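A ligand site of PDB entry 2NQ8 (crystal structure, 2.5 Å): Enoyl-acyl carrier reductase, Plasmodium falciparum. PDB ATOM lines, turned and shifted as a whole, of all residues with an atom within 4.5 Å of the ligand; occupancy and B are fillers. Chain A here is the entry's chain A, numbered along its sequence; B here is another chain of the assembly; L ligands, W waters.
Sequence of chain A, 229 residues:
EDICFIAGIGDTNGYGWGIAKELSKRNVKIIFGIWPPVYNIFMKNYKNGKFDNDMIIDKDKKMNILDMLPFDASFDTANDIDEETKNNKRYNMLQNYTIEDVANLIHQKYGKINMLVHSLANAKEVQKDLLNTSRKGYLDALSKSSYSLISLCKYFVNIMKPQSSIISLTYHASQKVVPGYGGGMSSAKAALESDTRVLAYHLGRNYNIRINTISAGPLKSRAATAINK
N of Leu 219 lies within hydrogen-bond range of O14 of the ligand (2.5 Å). O of Leu 219 lies within hydrogen-bond range of N7 of the ligand. O13 of the ligand lies within hydrogen-bond range of NZ of Lys 189. An oxygen (O5) of the ligand sits close to the backbone NH (N) of Ile 9 (3.2 Å). The backbone carbonyl oxygen (O) of Ile 9 lies close to an oxygen (O5) of the ligand, 3.0 Å away. N of Ala 73 lies within hydrogen-bond range of N4 of the ligand. A nitrogen (N8) of the ligand lies within hydrogen-bond range of the side-chain hydroxyl of Tyr 171, 3.0 Å away. OD1 of Asp 72 lies within hydrogen-bond range of N3 of the ligand (3.3 Å). The backbone NH (N) of Gly 10 is in hydrogen-bond range of an oxygen (O5) of the ligand, 3.3 Å away. The backbone carbonyl oxygen (O) of Leu 120 sits at hydrogen-bond distance from an oxygen (O12) of the ligand. O8 of the ligand sits at hydrogen-bond distance from OG of Ser 221.
O of Leu 169 lies within hydrogen-bond range of NZ of Lys 189, 2.8 Å away. OD2 of Asp 72 lies within hydrogen-bond range of NE1 of Trp 35 (3.5 Å). OD1 of Asp 72 lies within hydrogen-bond range of N of Ser 74 (2.9 Å). O of Thr 170 lies within hydrogen-bond range of N of Ala 216, at 3.1 Å. The backbone carbonyl oxygen of Gly 217 sits at hydrogen-bond distance from the side-chain hydroxyl of Tyr 15 (2.6 Å). The backbone NH of Gly 14 is in hydrogen-bond range of the side-chain carboxylate of Asp 11 (3.3 Å). ND2 of Asn 122 lies close to NZ of Lys 144, 3.2 Å away.
A nitrogen (N4) of the ligand sits close to the backbone carbonyl oxygen (O) of Phe 71 (3.3 Å). Residues that only touch the ligand: Gly 8 (3.5 Å), Gly 14 (3.5 Å), Tyr 15 (3.5 Å), Gly 16 (3.98 Å), Trp 35 (3.1 Å), Ser 74 (3.8 Å), Ser 119 (3.4 Å), Ala 121 (3.4 Å), Asn 122 (3.7 Å), Leu 169 (3.3 Å), Thr 170 (3.4 Å), Ala 216 (3.97 Å), Gly 217 (3.5 Å), Pro 218 (3.2 Å), Ala 223 (3.7 Å), Ala 224 (3.3 Å), Phe 3 of chain B (3.4 Å), Ile 4 of chain B (3.9 Å) and Ala 7 of chain B (3.4 Å). Hydrophobic or aromatic side chains within 4 Å of the ligand: Ile 9, Tyr 15, Trp 35, Phe 71, Ala 73, Leu 120, Ala 121, Leu 169, Tyr 171, Pro 218, Leu 219, Ala 223, Ala 224, Phe 3 of chain B, Ile 4 of chain B and Ala 7 of chain B. Of the 33 residues printed, 29 come within 4 Å of the ligand. The nearest printed residue that does not touch the ligand is Tyr 181 (4.1 Å).
Water W3 lies within hydrogen-bond range of an oxygen (O13) of the ligand (2.6 Å) and the side-chain hydroxyl of Tyr 181 (3.0 Å). Water W2 bridges O12 of the ligand (2.9 Å) and N of Leu 169 (3.1 Å). Water W1 bridges a nitrogen (N8) of the ligand and the side-chain hydroxyl of Tyr 171.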
ATOM      1  N   GLY A   8     -12.459  19.928  16.144  1.00  0.00           N
ATOM      2  CA  GLY A   8     -13.134  20.721  17.158  1.00  0.00           C
ATOM      3  C   GLY A   8     -13.638  19.892  18.317  1.00  0.00           C
ATOM      4  O   GLY A   8     -14.816  19.519  18.369  1.00  0.00           O
ATOM      5  N   ILE A   9     -12.755  19.606  19.259  1.00  0.00           N
ATOM      6  CA  ILE A   9     -13.091  18.818  20.425  1.00  0.00           C
ATOM      7  C   ILE A   9     -12.214  19.209  21.617  1.00  0.00           C
ATOM      8  O   ILE A   9     -11.165  19.822  21.450  1.00  0.00           O
ATOM      9  CB  ILE A   9     -12.942  17.294  20.124  1.00  0.00           C
ATOM     10  CG1 ILE A   9     -14.237  16.764  19.523  1.00  0.00           C
ATOM     11  CG2 ILE A   9     -12.622  16.501  21.380  1.00  0.00           C
ATOM     12  CD1 ILE A   9     -15.441  16.983  20.407  1.00  0.00           C
ATOM     13  N   GLY A  10     -12.703  18.882  22.806  1.00  0.00           N
ATOM     14  CA  GLY A  10     -11.989  19.178  24.036  1.00  0.00           C
ATOM     15  C   GLY A  10     -12.478  18.262  25.137  1.00  0.00           C
ATOM     16  O   GLY A  10     -11.753  17.935  26.066  1.00  0.00           O
ATOM     17  N   ASP A  11     -13.738  17.832  25.021  1.00  0.00           N
ATOM     18  CA  ASP A  11     -14.320  16.960  26.016  1.00  0.00           C
ATOM     19  C   ASP A  11     -15.428  16.105  25.403  1.00  0.00           C
ATOM     20  O   ASP A  11     -15.674  16.167  24.197  1.00  0.00           O
ATOM     21  CB  ASP A  11     -14.885  17.778  27.174  1.00  0.00           C
ATOM     22  CG  ASP A  11     -15.906  18.805  26.718  1.00  0.00           C
ATOM     23  OD1 ASP A  11     -16.903  18.407  26.068  1.00  0.00           O
ATOM     24  OD2 ASP A  11     -15.710  20.004  27.006  1.00  0.00           O
ATOM     25  N   GLY A  14     -19.547  17.822  24.236  1.00  0.00           N
ATOM     26  CA  GLY A  14     -19.862  18.632  23.073  1.00  0.00           C
ATOM     27  C   GLY A  14     -20.561  17.840  22.003  1.00  0.00           C
ATOM     28  O   GLY A  14     -20.907  16.672  22.210  1.00  0.00           O
ATOM     29  N   TYR A  15     -20.778  18.468  20.858  1.00  0.00           N
ATOM     30  CA  TYR A  15     -21.436  17.808  19.747  1.00  0.00           C
ATOM     31  C   TYR A  15     -20.478  16.876  19.011  1.00  0.00           C
ATOM     32  O   TYR A  15     -20.894  15.840  18.471  1.00  0.00           O
ATOM     33  CB  TYR A  15     -22.010  18.854  18.788  1.00  0.00           C
ATOM     34  CG  TYR A  15     -23.363  19.373  19.212  1.00  0.00           C
ATOM     35  CD1 TYR A  15     -24.374  18.503  19.612  1.00  0.00           C
ATOM     36  CD2 TYR A  15     -23.662  20.746  19.194  1.00  0.00           C
ATOM     37  CE1 TYR A  15     -25.634  18.954  19.971  1.00  0.00           C
ATOM     38  CE2 TYR A  15     -24.929  21.220  19.555  1.00  0.00           C
ATOM     39  CZ  TYR A  15     -25.909  20.310  19.937  1.00  0.00           C
ATOM     40  OH  TYR A  15     -27.176  20.743  20.286  1.00  0.00           O
ATOM     41  N   GLY A  16     -19.198  17.233  18.988  1.00  0.00           N
ATOM     42  CA  GLY A  16     -18.224  16.401  18.325  1.00  0.00           C
ATOM     43  C   GLY A  16     -18.315  14.966  18.815  1.00  0.00           C
ATOM     44  O   GLY A  16     -18.334  14.026  18.030  1.00  0.00           O
ATOM     45  N   TRP A  35      -7.798  21.165  19.780  1.00  0.00           N
ATOM     46  CA  TRP A  35      -7.146  22.461  19.894  1.00  0.00           C
ATOM     47  C   TRP A  35      -5.931  22.311  20.829  1.00  0.00           C
ATOM     48  O   TRP A  35      -6.086  22.032  22.016  1.00  0.00           O
ATOM     49  CB  TRP A  35      -8.145  23.467  20.462  1.00  0.00           C
ATOM     50  CG  TRP A  35      -7.657  24.897  20.508  1.00  0.00           C
ATOM     51  CD1 TRP A  35      -7.009  25.583  19.512  1.00  0.00           C
ATOM     52  CD2 TRP A  35      -7.885  25.833  21.561  1.00  0.00           C
ATOM     53  NE1 TRP A  35      -6.833  26.895  19.886  1.00  0.00           N
ATOM     54  CE2 TRP A  35      -7.359  27.078  21.133  1.00  0.00           C
ATOM     55  CE3 TRP A  35      -8.482  25.762  22.825  1.00  0.00           C
ATOM     56  CZ2 TRP A  35      -7.427  28.232  21.912  1.00  0.00           C
ATOM     57  CZ3 TRP A  35      -8.549  26.908  23.609  1.00  0.00           C
ATOM     58  CH2 TRP A  35      -8.021  28.122  23.146  1.00  0.00           C
ATOM     59  N   PHE A  71      -4.783  20.090  16.647  1.00  0.00           N
ATOM     60  CA  PHE A  71      -5.298  20.786  15.477  1.00  0.00           C
ATOM     61  C   PHE A  71      -5.727  22.207  15.811  1.00  0.00           C
ATOM     62  O   PHE A  71      -6.494  22.429  16.752  1.00  0.00           O
ATOM     63  CB  PHE A  71      -6.511  19.999  14.950  1.00  0.00           C
ATOM     64  CG  PHE A  71      -7.268  20.704  13.879  1.00  0.00           C
ATOM     65  CD1 PHE A  71      -6.913  20.546  12.534  1.00  0.00           C
ATOM     66  CD2 PHE A  71      -8.324  21.544  14.201  1.00  0.00           C
ATOM     67  CE1 PHE A  71      -7.608  21.215  11.528  1.00  0.00           C
ATOM     68  CE2 PHE A  71      -9.032  22.220  13.212  1.00  0.00           C
ATOM     69  CZ  PHE A  71      -8.678  22.062  11.866  1.00  0.00           C
ATOM     70  N   ASP A  72      -5.230  23.191  15.062  1.00  0.00           N
ATOM     71  CA  ASP A  72      -5.607  24.581  15.305  1.00  0.00           C
ATOM     72  C   ASP A  72      -6.163  25.213  14.028  1.00  0.00           C
ATOM     73  O   ASP A  72      -5.426  25.517  13.089  1.00  0.00           O
ATOM     74  CB  ASP A  72      -4.416  25.386  15.807  1.00  0.00           C
ATOM     75  CG  ASP A  72      -4.846  26.721  16.383  1.00  0.00           C
ATOM     76  OD1 ASP A  72      -5.678  27.391  15.750  1.00  0.00           O
ATOM     77  OD2 ASP A  72      -4.354  27.100  17.467  1.00  0.00           O
ATOM     78  N   ALA A  73      -7.481  25.433  14.024  1.00  0.00           N
ATOM     79  CA  ALA A  73      -8.187  25.987  12.873  1.00  0.00           C
ATOM     80  C   ALA A  73      -7.894  27.451  12.550  1.00  0.00           C
ATOM     81  O   ALA A  73      -8.544  28.038  11.676  1.00  0.00           O
ATOM     82  CB  ALA A  73      -9.676  25.785  13.067  1.00  0.00           C
ATOM     83  N   SER A  74      -6.937  28.042  13.248  1.00  0.00           N
ATOM     84  CA  SER A  74      -6.609  29.432  12.991  1.00  0.00           C
ATOM     85  C   SER A  74      -5.356  29.556  12.111  1.00  0.00           C
ATOM     86  O   SER A  74      -5.009  30.658  11.680  1.00  0.00           O
ATOM     87  CB  SER A  74      -6.398  30.187  14.309  1.00  0.00           C
ATOM     88  OG  SER A  74      -5.322  29.647  15.032  1.00  0.00           O
ATOM     89  N   SER A 119     -16.617  21.045  13.644  1.00  0.00           N
ATOM     90  CA  SER A 119     -17.362  21.206  14.888  1.00  0.00           C
ATOM     91  C   SER A 119     -16.617  22.074  15.895  1.00  0.00           C
ATOM     92  O   SER A 119     -16.371  21.667  17.015  1.00  0.00           O
ATOM     93  CB  SER A 119     -17.622  19.824  15.498  1.00  0.00           C
ATOM     94  OG  SER A 119     -18.484  19.912  16.620  1.00  0.00           O
ATOM     95  N   LEU A 120     -16.270  23.277  15.480  1.00  0.00           N
ATOM     96  CA  LEU A 120     -15.540  24.167  16.363  1.00  0.00           C
ATOM     97  C   LEU A 120     -15.990  25.602  16.143  1.00  0.00           C
ATOM     98  O   LEU A 120     -16.317  26.007  15.020  1.00  0.00           O
ATOM     99  CB  LEU A 120     -14.043  24.041  16.094  1.00  0.00           C
ATOM    100  CG  LEU A 120     -13.589  24.519  14.709  1.00  0.00           C
ATOM    101  CD1 LEU A 120     -13.266  26.004  14.793  1.00  0.00           C
ATOM    102  CD2 LEU A 120     -12.381  23.730  14.250  1.00  0.00           C
ATOM    103  N   ALA A 121     -16.013  26.365  17.224  1.00  0.00           N
ATOM    104  CA  ALA A 121     -16.420  27.768  17.186  1.00  0.00           C
ATOM    105  C   ALA A 121     -15.637  28.555  18.222  1.00  0.00           C
ATOM    106  O   ALA A 121     -15.341  28.046  19.311  1.00  0.00           O
ATOM    107  CB  ALA A 121     -17.911  27.880  17.448  1.00  0.00           C
ATOM    108  N   ASN A 122     -15.265  29.786  17.894  1.00  0.00           N
ATOM    109  CA  ASN A 122     -14.531  30.600  18.848  1.00  0.00           C
ATOM    110  C   ASN A 122     -14.636  32.073  18.585  1.00  0.00           C
ATOM    111  O   ASN A 122     -14.483  32.535  17.457  1.00  0.00           O
ATOM    112  CB  ASN A 122     -13.061  30.203  18.887  1.00  0.00           C
ATOM    113  CG  ASN A 122     -12.309  30.968  19.956  1.00  0.00           C
ATOM    114  OD1 ASN A 122     -12.557  30.797  21.154  1.00  0.00           O
ATOM    115  ND2 ASN A 122     -11.380  31.825  19.532  1.00  0.00           N
ATOM    116  N   LYS A 144     -11.812  32.055  13.049  1.00  0.00           N
ATOM    117  CA  LYS A 144     -11.910  30.790  13.766  1.00  0.00           C
ATOM    118  C   LYS A 144     -13.204  30.008  13.523  1.00  0.00           C
ATOM    119  O   LYS A 144     -13.186  28.780  13.418  1.00  0.00           O
ATOM    120  CB  LYS A 144     -11.788  31.015  15.275  1.00  0.00           C
ATOM    121  CG  LYS A 144     -10.384  30.907  15.859  1.00  0.00           C
ATOM    122  CD  LYS A 144      -9.526  32.120  15.557  1.00  0.00           C
ATOM    123  CE  LYS A 144      -8.285  32.127  16.457  1.00  0.00           C
ATOM    124  NZ  LYS A 144      -8.649  32.147  17.909  1.00  0.00           N
ATOM    125  N   LEU A 169     -21.459  22.713  12.182  1.00  0.00           N
ATOM    126  CA  LEU A 169     -22.533  23.066  13.130  1.00  0.00           C
ATOM    127  C   LEU A 169     -22.793  24.570  13.152  1.00  0.00           C
ATOM    128  O   LEU A 169     -21.867  25.375  13.201  1.00  0.00           O
ATOM    129  CB  LEU A 169     -22.174  22.600  14.553  1.00  0.00           C
ATOM    130  CG  LEU A 169     -22.271  21.117  14.956  1.00  0.00           C
ATOM    131  CD1 LEU A 169     -23.727  20.681  14.988  1.00  0.00           C
ATOM    132  CD2 LEU A 169     -21.482  20.259  13.982  1.00  0.00           C
ATOM    133  N   THR A 170     -24.063  24.960  13.131  1.00  0.00           N
ATOM    134  CA  THR A 170     -24.405  26.381  13.148  1.00  0.00           C
ATOM    135  C   THR A 170     -25.542  26.630  14.133  1.00  0.00           C
ATOM    136  O   THR A 170     -26.009  25.694  14.795  1.00  0.00           O
ATOM    137  CB  THR A 170     -24.836  26.854  11.738  1.00  0.00           C
ATOM    138  OG1 THR A 170     -24.981  28.283  11.739  1.00  0.00           O
ATOM    139  CG2 THR A 170     -26.158  26.201  11.337  1.00  0.00           C
ATOM    140  N   TYR A 171     -25.972  27.882  14.244  1.00  0.00           N
ATOM    141  CA  TYR A 171     -27.049  28.241  15.163  1.00  0.00           C
ATOM    142  C   TYR A 171     -28.001  29.284  14.550  1.00  0.00           C
ATOM    143  O   TYR A 171     -27.569  30.255  13.900  1.00  0.00           O
ATOM    144  CB  TYR A 171     -26.428  28.748  16.487  1.00  0.00           C
ATOM    145  CG  TYR A 171     -27.395  29.243  17.519  1.00  0.00           C
ATOM    146  CD1 TYR A 171     -28.592  28.563  17.790  1.00  0.00           C
ATOM    147  CD2 TYR A 171     -27.130  30.412  18.236  1.00  0.00           C
ATOM    148  CE1 TYR A 171     -29.493  29.033  18.759  1.00  0.00           C
ATOM    149  CE2 TYR A 171     -28.004  30.889  19.211  1.00  0.00           C
ATOM    150  CZ  TYR A 171     -29.187  30.193  19.471  1.00  0.00           C
ATOM    151  OH  TYR A 171     -30.052  30.669  20.441  1.00  0.00           O
ATOM    152  N   TYR A 181     -25.905  36.259  22.319  1.00  0.00           N
ATOM    153  CA  TYR A 181     -25.003  35.509  21.448  1.00  0.00           C
ATOM    154  C   TYR A 181     -24.217  36.565  20.692  1.00  0.00           C
ATOM    155  O   TYR A 181     -24.573  36.890  19.556  1.00  0.00           O
ATOM    156  CB  TYR A 181     -25.827  34.643  20.486  1.00  0.00           C
ATOM    157  CG  TYR A 181     -25.025  33.602  19.741  1.00  0.00           C
ATOM    158  CD1 TYR A 181     -24.556  32.461  20.386  1.00  0.00           C
ATOM    159  CD2 TYR A 181     -24.769  33.748  18.367  1.00  0.00           C
ATOM    160  CE1 TYR A 181     -23.852  31.473  19.678  1.00  0.00           C
ATOM    161  CE2 TYR A 181     -24.075  32.770  17.659  1.00  0.00           C
ATOM    162  CZ  TYR A 181     -23.611  31.643  18.312  1.00  0.00           C
ATOM    163  OH  TYR A 181     -22.933  30.679  17.591  1.00  0.00           O
ATOM    164  N   LYS A 189     -21.854  32.660  12.117  1.00  0.00           N
ATOM    165  CA  LYS A 189     -22.789  31.615  11.761  1.00  0.00           C
ATOM    166  C   LYS A 189     -23.564  31.983  10.477  1.00  0.00           C
ATOM    167  O   LYS A 189     -23.980  31.103   9.719  1.00  0.00           O
ATOM    168  CB  LYS A 189     -23.730  31.341  12.935  1.00  0.00           C
ATOM    169  CG  LYS A 189     -23.015  30.749  14.159  1.00  0.00           C
ATOM    170  CD  LYS A 189     -22.225  29.474  13.807  1.00  0.00           C
ATOM    171  CE  LYS A 189     -21.777  28.752  15.074  1.00  0.00           C
ATOM    172  NZ  LYS A 189     -20.951  27.506  14.829  1.00  0.00           N
ATOM    173  N   ALA A 216     -28.116  23.413  15.260  1.00  0.00           N
ATOM    174  CA  ALA A 216     -28.505  22.724  16.475  1.00  0.00           C
ATOM    175  C   ALA A 216     -29.170  23.539  17.548  1.00  0.00           C
ATOM    176  O   ALA A 216     -29.085  24.768  17.565  1.00  0.00           O
ATOM    177  CB  ALA A 216     -27.290  22.019  17.047  1.00  0.00           C
ATOM    178  N   GLY A 217     -29.847  22.819  18.449  1.00  0.00           N
ATOM    179  CA  GLY A 217     -30.508  23.428  19.585  1.00  0.00           C
ATOM    180  C   GLY A 217     -29.479  23.487  20.698  1.00  0.00           C
ATOM    181  O   GLY A 217     -28.331  23.077  20.486  1.00  0.00           O
ATOM    182  N   PRO A 218     -29.843  23.975  21.892  1.00  0.00           N
ATOM    183  CA  PRO A 218     -28.908  24.070  23.012  1.00  0.00           C
ATOM    184  C   PRO A 218     -28.380  22.775  23.613  1.00  0.00           C
ATOM    185  O   PRO A 218     -29.128  21.803  23.801  1.00  0.00           O
ATOM    186  CB  PRO A 218     -29.683  24.902  24.020  1.00  0.00           C
ATOM    187  CG  PRO A 218     -31.092  24.417  23.803  1.00  0.00           C
ATOM    188  CD  PRO A 218     -31.192  24.407  22.303  1.00  0.00           C
ATOM    189  N   LEU A 219     -27.089  22.776  23.903  1.00  0.00           N
ATOM    190  CA  LEU A 219     -26.401  21.645  24.530  1.00  0.00           C
ATOM    191  C   LEU A 219     -25.439  22.280  25.516  1.00  0.00           C
ATOM    192  O   LEU A 219     -24.662  23.175  25.160  1.00  0.00           O
ATOM    193  CB  LEU A 219     -25.611  20.828  23.503  1.00  0.00           C
ATOM    194  CG  LEU A 219     -25.001  19.525  24.047  1.00  0.00           C
ATOM    195  CD1 LEU A 219     -26.125  18.546  24.385  1.00  0.00           C
ATOM    196  CD2 LEU A 219     -24.071  18.911  23.019  1.00  0.00           C
ATOM    197  N   SER A 221     -22.380  22.196  26.941  1.00  0.00           N
ATOM    198  CA  SER A 221     -21.047  21.643  26.775  1.00  0.00           C
ATOM    199  C   SER A 221     -20.039  22.383  27.667  1.00  0.00           C
ATOM    200  O   SER A 221     -20.037  22.214  28.888  1.00  0.00           O
ATOM    201  CB  SER A 221     -20.629  21.739  25.310  1.00  0.00           C
ATOM    202  OG  SER A 221     -20.840  23.047  24.816  1.00  0.00           O
ATOM    203  N   ARG A 222     -19.205  23.208  27.043  1.00  0.00           N
ATOM    204  CA  ARG A 222     -18.214  23.996  27.755  1.00  0.00           C
ATOM    205  C   ARG A 222     -17.978  25.290  26.990  1.00  0.00           C
ATOM    206  O   ARG A 222     -17.815  26.361  27.578  1.00  0.00           O
ATOM    207  CB  ARG A 222     -16.900  23.229  27.896  1.00  0.00           C
ATOM    208  CG  ARG A 222     -15.854  23.956  28.733  1.00  0.00           C
ATOM    209  CD  ARG A 222     -14.528  23.218  28.756  1.00  0.00           C
ATOM    210  NE  ARG A 222     -13.538  23.917  29.578  1.00  0.00           N
ATOM    211  CZ  ARG A 222     -13.125  25.162  29.349  1.00  0.00           C
ATOM    212  NH1 ARG A 222     -13.616  25.858  28.337  1.00  0.00           N
ATOM    213  NH2 ARG A 222     -12.212  25.722  30.147  1.00  0.00           N
ATOM    214  N   ALA A 223     -17.957  25.185  25.664  1.00  0.00           N
ATOM    215  CA  ALA A 223     -17.757  26.338  24.798  1.00  0.00           C
ATOM    216  C   ALA A 223     -19.070  27.119  24.767  1.00  0.00           C
ATOM    217  O   ALA A 223     -19.110  28.291  24.378  1.00  0.00           O
ATOM    218  CB  ALA A 223     -17.384  25.884  23.391  1.00  0.00           C
ATOM    219  N   ALA A 224     -20.138  26.464  25.197  1.00  0.00           N
ATOM    220  CA  ALA A 224     -21.467  27.058  25.228  1.00  0.00           C
ATOM    221  C   ALA A 224     -21.704  27.760  26.569  1.00  0.00           C
ATOM    222  O   ALA A 224     -22.384  28.786  26.628  1.00  0.00           O
ATOM    223  CB  ALA A 224     -22.526  25.990  24.987  1.00  0.00           C
ATOM    224  N   PHE B   3     -26.061  32.033  29.995  1.00  0.00           N
ATOM    225  CA  PHE B   3     -26.882  32.164  28.796  1.00  0.00           C
ATOM    226  C   PHE B   3     -27.389  30.804  28.318  1.00  0.00           C
ATOM    227  O   PHE B   3     -28.542  30.667  27.913  1.00  0.00           O
ATOM    228  CB  PHE B   3     -26.040  32.824  27.702  1.00  0.00           C
ATOM    229  CG  PHE B   3     -26.573  32.637  26.308  1.00  0.00           C
ATOM    230  CD1 PHE B   3     -27.627  33.409  25.836  1.00  0.00           C
ATOM    231  CD2 PHE B   3     -26.008  31.686  25.474  1.00  0.00           C
ATOM    232  CE1 PHE B   3     -28.104  33.231  24.549  1.00  0.00           C
ATOM    233  CE2 PHE B   3     -26.476  31.498  24.188  1.00  0.00           C
ATOM    234  CZ  PHE B   3     -27.531  32.279  23.710  1.00  0.00           C
ATOM    235  N   ILE B   4     -26.511  29.822  28.392  1.00  0.00           N
ATOM    236  CA  ILE B   4     -26.828  28.476  27.952  1.00  0.00           C
ATOM    237  C   ILE B   4     -27.948  27.777  28.733  1.00  0.00           C
ATOM    238  O   ILE B   4     -28.783  27.081  28.148  1.00  0.00           O
ATOM    239  CB  ILE B   4     -25.554  27.594  27.977  1.00  0.00           C
ATOM    240  CG1 ILE B   4     -25.819  26.283  27.231  1.00  0.00           C
ATOM    241  CG2 ILE B   4     -25.140  27.327  29.413  1.00  0.00           C
ATOM    242  CD1 ILE B   4     -26.133  26.481  25.767  1.00  0.00           C
ATOM    243  N   ALA B   7     -31.332  29.246  27.656  1.00  0.00           N
ATOM    244  CA  ALA B   7     -31.701  28.753  26.332  1.00  0.00           C
ATOM    245  C   ALA B   7     -32.299  27.356  26.396  1.00  0.00           C
ATOM    246  O   ALA B   7     -33.296  27.078  25.735  1.00  0.00           O
ATOM    247  CB  ALA B   7     -30.494  28.770  25.415  1.00  0.00           C
HETATM  248  P1  LIG L   1     -17.251  21.308  21.830  1.00  0.00           P
HETATM  249  O1  LIG L   1     -17.421  20.405  20.608  1.00  0.00           O
HETATM  250  O2  LIG L   1     -17.871  21.538  23.168  1.00  0.00           O
HETATM  251  O3  LIG L   1     -16.661  22.820  21.432  1.00  0.00           O
HETATM  252  C1  LIG L   1     -16.010  23.169  20.157  1.00  0.00           C
HETATM  253  C2  LIG L   1     -14.525  23.389  20.060  1.00  0.00           C
HETATM  254  O4  LIG L   1     -14.122  24.783  19.729  1.00  0.00           O
HETATM  255  C3  LIG L   1     -13.754  23.179  21.338  1.00  0.00           C
HETATM  256  O5  LIG L   1     -13.429  21.815  21.428  1.00  0.00           O
HETATM  257  C4  LIG L   1     -12.518  24.023  21.165  1.00  0.00           C
HETATM  258  O6  LIG L   1     -11.285  23.338  21.435  1.00  0.00           O
HETATM  259  C5  LIG L   1     -12.728  24.498  19.742  1.00  0.00           C
HETATM  260  N1  LIG L   1     -11.561  25.524  19.520  1.00  0.00           N
HETATM  261  C6  LIG L   1     -11.526  26.869  19.321  1.00  0.00           C
HETATM  262  N2  LIG L   1     -10.687  27.255  18.336  1.00  0.00           N
HETATM  263  C7  LIG L   1     -10.198  26.136  17.907  1.00  0.00           C
HETATM  264  C8  LIG L   1      -9.236  25.958  16.848  1.00  0.00           C
HETATM  265  N3  LIG L   1      -8.854  26.931  16.319  1.00  0.00           N
HETATM  266  N4  LIG L   1      -8.849  24.678  16.528  1.00  0.00           N
HETATM  267  C9  LIG L   1      -9.330  23.576  17.184  1.00  0.00           C
HETATM  268  N5  LIG L   1     -10.230  23.684  18.184  1.00  0.00           N
HETATM  269  C10 LIG L   1     -10.704  25.020  18.586  1.00  0.00           C
HETATM  270  O7  LIG L   1     -18.810  21.481  21.323  1.00  0.00           O
HETATM  271  P2  LIG L   1     -19.922  22.612  21.414  1.00  0.00           P
HETATM  272  O8  LIG L   1     -21.384  22.343  21.436  1.00  0.00           O
HETATM  273  O9  LIG L   1     -19.293  23.890  20.956  1.00  0.00           O
HETATM  274  O10 LIG L   1     -20.072  22.216  19.831  1.00  0.00           O
HETATM  275  C11 LIG L   1     -19.177  22.607  18.757  1.00  0.00           C
HETATM  276  C12 LIG L   1     -19.926  23.184  17.536  1.00  0.00           C
HETATM  277  O11 LIG L   1     -21.373  23.108  17.758  1.00  0.00           O
HETATM  278  C13 LIG L   1     -19.637  24.653  17.160  1.00  0.00           C
HETATM  279  O12 LIG L   1     -19.449  24.921  15.775  1.00  0.00           O
HETATM  280  C14 LIG L   1     -20.825  25.357  17.792  1.00  0.00           C
HETATM  281  O13 LIG L   1     -21.147  26.729  17.550  1.00  0.00           O
HETATM  282  C15 LIG L   1     -21.944  24.417  17.466  1.00  0.00           C
HETATM  283  N6  LIG L   1     -23.170  24.713  18.288  1.00  0.00           N
HETATM  284  C16 LIG L   1     -23.284  24.339  19.669  1.00  0.00           C
HETATM  285  C17 LIG L   1     -24.433  24.721  20.417  1.00  0.00           C
HETATM  286  C18 LIG L   1     -24.616  24.321  21.936  1.00  0.00           C
HETATM  287  O14 LIG L   1     -25.721  24.350  22.511  1.00  0.00           O
HETATM  288  N7  LIG L   1     -23.475  23.945  22.541  1.00  0.00           N
HETATM  289  C19 LIG L   1     -25.460  25.516  19.769  1.00  0.00           C
HETATM  290  C20 LIG L   1     -25.354  25.840  18.385  1.00  0.00           C
HETATM  291  C21 LIG L   1     -24.213  25.451  17.645  1.00  0.00           C
HETATM  292  C22 LIG L   1     -25.593  26.867  20.568  1.00  0.00           C
HETATM  293  O15 LIG L   1     -24.568  27.554  20.753  1.00  0.00           O
HETATM  294  N8  LIG L   1     -29.295  28.365  22.223  1.00  0.00           N
HETATM  295  C23 LIG L   1     -28.150  29.074  22.416  1.00  0.00           C
HETATM  296  C24 LIG L   1     -26.930  28.619  21.871  1.00  0.00           C
HETATM  297  C25 LIG L   1     -26.927  27.389  21.139  1.00  0.00           C
HETATM  298  C26 LIG L   1     -28.150  26.671  20.972  1.00  0.00           C
HETATM  299  C27 LIG L   1     -29.345  27.184  21.531  1.00  0.00           C
HETATM  300  O   HOH W   1     -32.060  28.335  21.226  1.00  0.00           O
HETATM  301  O   HOH W   2     -18.905  24.280  12.979  1.00  0.00           O
HETATM  302  O   HOH W   3     -22.282  28.314  19.250  1.00  0.00           O
